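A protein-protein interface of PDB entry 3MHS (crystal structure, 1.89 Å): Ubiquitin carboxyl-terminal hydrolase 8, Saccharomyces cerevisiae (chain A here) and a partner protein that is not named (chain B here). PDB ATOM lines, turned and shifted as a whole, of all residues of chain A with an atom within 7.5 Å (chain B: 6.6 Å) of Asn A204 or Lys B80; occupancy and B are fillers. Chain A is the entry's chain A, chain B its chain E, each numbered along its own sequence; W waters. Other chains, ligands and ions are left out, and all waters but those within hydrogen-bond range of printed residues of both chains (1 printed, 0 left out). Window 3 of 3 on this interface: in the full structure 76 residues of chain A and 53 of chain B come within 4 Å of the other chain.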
ATOM      1  N   THR A 128     -20.858  21.688  19.886  1.00  0.00           N
ATOM      2  CA  THR A 128     -20.359  21.589  18.522  1.00  0.00           C
ATOM      3  C   THR A 128     -19.730  20.224  18.282  1.00  0.00           C
ATOM      4  O   THR A 128     -19.877  19.660  17.203  1.00  0.00           O
ATOM      5  CB  THR A 128     -19.336  22.693  18.202  1.00  0.00           C
ATOM      6  OG1 THR A 128     -19.829  23.947  18.684  1.00  0.00           O
ATOM      7  CG2 THR A 128     -19.096  22.793  16.681  1.00  0.00           C
ATOM      8  N   LYS A 129     -19.007  19.716  19.275  1.00  0.00           N
ATOM      9  CA  LYS A 129     -18.349  18.434  19.140  1.00  0.00           C
ATOM     10  C   LYS A 129     -19.335  17.294  19.333  1.00  0.00           C
ATOM     11  O   LYS A 129     -19.101  16.232  18.792  1.00  0.00           O
ATOM     12  CB  LYS A 129     -17.234  18.243  20.187  1.00  0.00           C
ATOM     13  CG  LYS A 129     -15.935  19.005  19.943  1.00  0.00           C
ATOM     14  CD  LYS A 129     -14.956  18.855  21.149  1.00  0.00           C
ATOM     15  CE  LYS A 129     -14.008  17.661  20.999  1.00  0.00           C
ATOM     16  NZ  LYS A 129     -12.911  17.701  22.022  1.00  0.00           N
ATOM     17  N   THR A 130     -20.411  17.497  20.111  1.00  0.00           N
ATOM     18  CA  THR A 130     -21.278  16.374  20.528  1.00  0.00           C
ATOM     19  C   THR A 130     -22.803  16.588  20.494  1.00  0.00           C
ATOM     20  O   THR A 130     -23.296  17.713  20.608  1.00  0.00           O
ATOM     21  CB  THR A 130     -20.896  15.867  21.941  1.00  0.00           C
ATOM     22  OG1 THR A 130     -21.417  16.741  22.951  1.00  0.00           O
ATOM     23  CG2 THR A 130     -19.397  15.771  22.083  1.00  0.00           C
ATOM     24  N   MET A 131     -23.528  15.467  20.391  1.00  0.00           N
ATOM     25  CA  MET A 131     -25.003  15.439  20.350  1.00  0.00           C
ATOM     26  C   MET A 131     -25.563  14.580  21.460  1.00  0.00           C
ATOM     27  O   MET A 131     -24.847  13.773  22.012  1.00  0.00           O
ATOM     28  CB  MET A 131     -25.487  14.878  19.009  1.00  0.00           C
ATOM     29  CG  MET A 131     -25.111  13.428  18.731  1.00  0.00           C
ATOM     30  SD  MET A 131     -25.770  12.852  17.140  1.00  0.00           S
ATOM     31  CE  MET A 131     -25.039  14.070  16.050  1.00  0.00           C
ATOM     32  N   HIS A 197     -19.154   1.376  21.910  1.00  0.00           N
ATOM     33  CA  HIS A 197     -19.319   2.368  20.832  1.00  0.00           C
ATOM     34  C   HIS A 197     -20.541   2.036  19.997  1.00  0.00           C
ATOM     35  O   HIS A 197     -21.400   2.898  19.751  1.00  0.00           O
ATOM     36  CB  HIS A 197     -18.030   2.373  19.976  1.00  0.00           C
ATOM     37  CG  HIS A 197     -17.973   3.443  18.936  1.00  0.00           C
ATOM     38  ND1 HIS A 197     -16.779   3.875  18.397  1.00  0.00           N
ATOM     39  CD2 HIS A 197     -18.946   4.159  18.325  1.00  0.00           C
ATOM     40  CE1 HIS A 197     -17.021   4.805  17.487  1.00  0.00           C
ATOM     41  NE2 HIS A 197     -18.326   5.003  17.430  1.00  0.00           N
ATOM     42  N   ALA A 202     -22.539   5.288  17.556  1.00  0.00           N
ATOM     43  CA  ALA A 202     -22.624   4.796  16.190  1.00  0.00           C
ATOM     44  C   ALA A 202     -21.227   4.707  15.617  1.00  0.00           C
ATOM     45  O   ALA A 202     -20.485   5.676  15.674  1.00  0.00           O
ATOM     46  CB  ALA A 202     -23.490   5.721  15.321  1.00  0.00           C
ATOM     47  N   LEU A 203     -20.871   3.540  15.091  1.00  0.00           N
ATOM     48  CA  LEU A 203     -19.613   3.372  14.383  1.00  0.00           C
ATOM     49  C   LEU A 203     -19.774   4.075  13.056  1.00  0.00           C
ATOM     50  O   LEU A 203     -20.858   4.065  12.482  1.00  0.00           O
ATOM     51  CB  LEU A 203     -19.309   1.896  14.114  1.00  0.00           C
ATOM     52  CG  LEU A 203     -18.982   0.978  15.278  1.00  0.00           C
ATOM     53  CD1 LEU A 203     -18.452  -0.370  14.717  1.00  0.00           C
ATOM     54  CD2 LEU A 203     -17.962   1.614  16.231  1.00  0.00           C
ATOM     55  N   ASN A 204     -18.718   4.693  12.551  1.00  0.00           N
ATOM     56  CA  ASN A 204     -18.837   5.327  11.244  1.00  0.00           C
ATOM     57  C   ASN A 204     -19.106   4.230  10.209  1.00  0.00           C
ATOM     58  O   ASN A 204     -18.307   3.299  10.078  1.00  0.00           O
ATOM     59  CB  ASN A 204     -17.580   6.136  10.889  1.00  0.00           C
ATOM     60  CG  ASN A 204     -17.602   7.549  11.470  1.00  0.00           C
ATOM     61  OD1 ASN A 204     -16.554   8.124  11.773  1.00  0.00           O
ATOM     62  ND2 ASN A 204     -18.794   8.116  11.611  1.00  0.00           N
ATOM     63  N   THR A 205     -20.236   4.305   9.505  1.00  0.00           N
ATOM     64  CA  THR A 205     -21.193   5.405   9.630  1.00  0.00           C
ATOM     65  C   THR A 205     -22.627   4.898   9.423  1.00  0.00           C
ATOM     66  O   THR A 205     -23.220   5.051   8.351  1.00  0.00           O
ATOM     67  CB  THR A 205     -20.847   6.555   8.633  1.00  0.00           C
ATOM     68  OG1 THR A 205     -21.778   7.638   8.784  1.00  0.00           O
ATOM     69  CG2 THR A 205     -20.851   6.053   7.183  1.00  0.00           C
ATOM     70  N   VAL B  77     -22.633  12.005  22.319  1.00  0.00           N
ATOM     71  CA  VAL B  77     -22.034  11.276  21.236  1.00  0.00           C
ATOM     72  C   VAL B  77     -21.248  12.213  20.335  1.00  0.00           C
ATOM     73  O   VAL B  77     -21.736  13.277  19.932  1.00  0.00           O
ATOM     74  CB  VAL B  77     -23.126  10.524  20.454  1.00  0.00           C
ATOM     75  CG1 VAL B  77     -22.537   9.832  19.198  1.00  0.00           C
ATOM     76  CG2 VAL B  77     -23.818   9.492  21.400  1.00  0.00           C
ATOM     77  N   CYS B  78     -20.016  11.832  20.038  1.00  0.00           N
ATOM     78  CA  CYS B  78     -19.173  12.644  19.183  1.00  0.00           C
ATOM     79  C   CYS B  78     -19.758  12.776  17.765  1.00  0.00           C
ATOM     80  O   CYS B  78     -20.090  11.776  17.111  1.00  0.00           O
ATOM     81  CB  CYS B  78     -17.788  12.038  19.099  1.00  0.00           C
ATOM     82  SG  CYS B  78     -16.664  13.033  18.063  1.00  0.00           S
ATOM     83  N   GLU B  79     -19.819  14.014  17.286  1.00  0.00           N
ATOM     84  CA  GLU B  79     -20.360  14.307  15.969  1.00  0.00           C
ATOM     85  C   GLU B  79     -19.456  13.728  14.886  1.00  0.00           C
ATOM     86  O   GLU B  79     -19.929  13.352  13.824  1.00  0.00           O
ATOM     87  CB  GLU B  79     -20.509  15.826  15.785  1.00  0.00           C
ATOM     88  CG  GLU B  79     -21.640  16.451  16.636  1.00  0.00           C
ATOM     89  CD  GLU B  79     -23.003  16.383  15.951  1.00  0.00           C
ATOM     90  OE1 GLU B  79     -23.083  15.744  14.884  1.00  0.00           O
ATOM     91  OE2 GLU B  79     -23.983  16.981  16.457  1.00  0.00           O
ATOM     92  N   LYS B  80     -18.159  13.662  15.151  1.00  0.00           N
ATOM     93  CA  LYS B  80     -17.204  13.243  14.139  1.00  0.00           C
ATOM     94  C   LYS B  80     -17.065  11.727  14.022  1.00  0.00           C
ATOM     95  O   LYS B  80     -17.036  11.187  12.923  1.00  0.00           O
ATOM     96  CB  LYS B  80     -15.839  13.836  14.454  1.00  0.00           C
ATOM     97  CG  LYS B  80     -15.667  15.295  14.048  1.00  0.00           C
ATOM     98  CD  LYS B  80     -14.370  15.853  14.654  1.00  0.00           C
ATOM     99  CE  LYS B  80     -13.953  17.174  14.024  1.00  0.00           C
ATOM    100  NZ  LYS B  80     -12.469  17.392  14.141  1.00  0.00           N
ATOM    101  N   CYS B  81     -16.931  11.051  15.158  1.00  0.00           N
ATOM    102  CA  CYS B  81     -16.630   9.624  15.176  1.00  0.00           C
ATOM    103  C   CYS B  81     -17.721   8.739  15.823  1.00  0.00           C
ATOM    104  O   CYS B  81     -17.605   7.526  15.807  1.00  0.00           O
ATOM    105  CB  CYS B  81     -15.292   9.370  15.875  1.00  0.00           C
ATOM    106  SG  CYS B  81     -15.337   9.550  17.649  1.00  0.00           S
ATOM    107  N   GLY B  82     -18.759   9.349  16.377  1.00  0.00           N
ATOM    108  CA  GLY B  82     -19.883   8.610  16.941  1.00  0.00           C
ATOM    109  C   GLY B  82     -19.631   7.922  18.281  1.00  0.00           C
ATOM    110  O   GLY B  82     -20.468   7.144  18.705  1.00  0.00           O
ATOM    111  N   LYS B  83     -18.511   8.211  18.955  1.00  0.00           N
ATOM    112  CA  LYS B  83     -18.211   7.579  20.253  1.00  0.00           C
ATOM    113  C   LYS B  83     -19.092   8.117  21.341  1.00  0.00           C
ATOM    114  O   LYS B  83     -19.295   9.325  21.415  1.00  0.00           O
ATOM    115  CB  LYS B  83     -16.764   7.845  20.694  1.00  0.00           C
ATOM    116  CG  LYS B  83     -15.753   6.833  20.166  1.00  0.00           C
ATOM    117  CD  LYS B  83     -14.452   6.960  20.910  1.00  0.00           C
ATOM    118  CE  LYS B  83     -13.421   6.008  20.381  1.00  0.00           C
ATOM    119  NZ  LYS B  83     -12.367   5.811  21.408  1.00  0.00           N
ATOM    120  N   HIS B  93     -11.463  15.006  24.133  1.00  0.00           N
ATOM    121  CA  HIS B  93     -11.577  13.984  23.094  1.00  0.00           C
ATOM    122  C   HIS B  93     -11.184  14.475  21.663  1.00  0.00           C
ATOM    123  O   HIS B  93     -11.776  15.417  21.160  1.00  0.00           O
ATOM    124  CB  HIS B  93     -12.999  13.385  23.118  1.00  0.00           C
ATOM    125  CG  HIS B  93     -13.330  12.630  21.887  1.00  0.00           C
ATOM    126  ND1 HIS B  93     -12.795  11.391  21.603  1.00  0.00           N
ATOM    127  CD2 HIS B  93     -14.050  12.989  20.804  1.00  0.00           C
ATOM    128  CE1 HIS B  93     -13.190  11.013  20.403  1.00  0.00           C
ATOM    129  NE2 HIS B  93     -13.937  11.976  19.890  1.00  0.00           N
ATOM    130  N   GLU B  95      -9.780  13.212  17.362  1.00  0.00           N
ATOM    131  CA  GLU B  95      -9.926  12.161  16.332  1.00  0.00           C
ATOM    132  C   GLU B  95      -8.609  11.431  16.044  1.00  0.00           C
ATOM    133  O   GLU B  95      -8.366  10.304  16.493  1.00  0.00           O
ATOM    134  CB  GLU B  95     -10.458  12.758  15.018  1.00  0.00           C
ATOM    135  CG  GLU B  95     -11.812  13.451  15.138  1.00  0.00           C
ATOM    136  CD  GLU B  95     -12.860  12.574  15.792  1.00  0.00           C
ATOM    137  OE1 GLU B  95     -13.167  11.513  15.206  1.00  0.00           O
ATOM    138  OE2 GLU B  95     -13.332  12.939  16.903  1.00  0.00           O
HETATM  139  O   HOH W   1     -16.763   5.629  14.053  1.00  0.00           O
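Of the 9 printed residues of chain B, 8 touch a printed residue of chain A.
Printed residues of chain B that touch a printed residue of chain A: Val B77, Cys B78, Glu B79, Lys B80, Cys B81, Gly B82, Lys B83 and His B93.
Among the printed residues, 15 pairs touch across the chains.
O of Thr A128 touches CG of Glu B79, at 3.7 Å.
Lys A129 touches Cys B78.
Thr A130 touches Val B77 (CA to O, 3.2 Å).
N of Thr A130 touches CG of Glu B79, 3.8 Å away.
Met A131 touches Glu B79.
His A197 touches Lys B83 (NE2 to N, 3.6 Å).
CA of Cys B81 touches OD1 of Asn A204, at 3.7 Å.
Of chain B, only Lys B80 and Cys B81 come within 4 Å of Asn A204.
Lys B80 touches just one residue of chain A: Asn A204.
Of the printed residues of chain A, His B93 touches Lys A129 (2.7 Å).
Of the printed residues of chain B, Thr A130 touches Val B77 and Glu B79.
Of the printed residues of chain B, His A197 touches Cys B81 (3.1 Å), Gly B82 (3.3 Å) and Lys B83 (3.6 Å).
Of the printed residues of chain B, Lys A129 touches Cys B78 (3.6 Å), Glu B79 (2.8 Å) and His B93 (2.7 Å).
Of the printed residues of chain B, Met A131 touches Val B77 (2.8 Å) and Glu B79 (2.8 Å).
Thr A205 touches none of the printed residues of chain B.
The nearest residue of chain B that does not touch Asn A204 is Gly B82 (4.9 Å).
Water W1 lies within hydrogen-bond range of N of Asn A204 (2.6 Å) and O of Cys B81 (2.7 Å).
The backbone NH of Lys B83 sits close to the side-chain sulfur of Cys B81, at 3.7 Å.
The backbone carbonyl oxygen (O) of Lys B83 sits at hydrogen-bond distance from the backbone NH (N) of Cys B78.
O of Ala A202 sits at hydrogen-bond distance from NE2 of His A197.
SG of Cys B78 sits close to N of Lys B80 (3.3 Å).
The backbone carbonyl oxygen of Lys B80 sits close to the side-chain amide oxygen of Asn A204 (3.3 Å).
A ring nitrogen (NE2) of His A197 sits at hydrogen-bond distance from the backbone carbonyl oxygen (O) of Gly B82, 3.3 Å away.
The backbone carbonyl oxygen of Cys B81 sits close to the backbone carbonyl oxygen of Ala A202 (3.4 Å).
A ring nitrogen (NE2) of His A197 is in hydrogen-bond range of the backbone carbonyl oxygen of Cys B81.
O of His B93 sits at hydrogen-bond distance from NZ of Lys A129, at 2.7 Å.
N of Ala A202 lies within hydrogen-bond range of O of Gly B82, at 3.0 Å.
The backbone carbonyl oxygen (O) of Lys A129 sits at hydrogen-bond distance from the backbone NH (N) of Glu B79 (2.8 Å).
O of Met A131 sits at hydrogen-bond distance from N of Val B77, at 2.8 Å.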
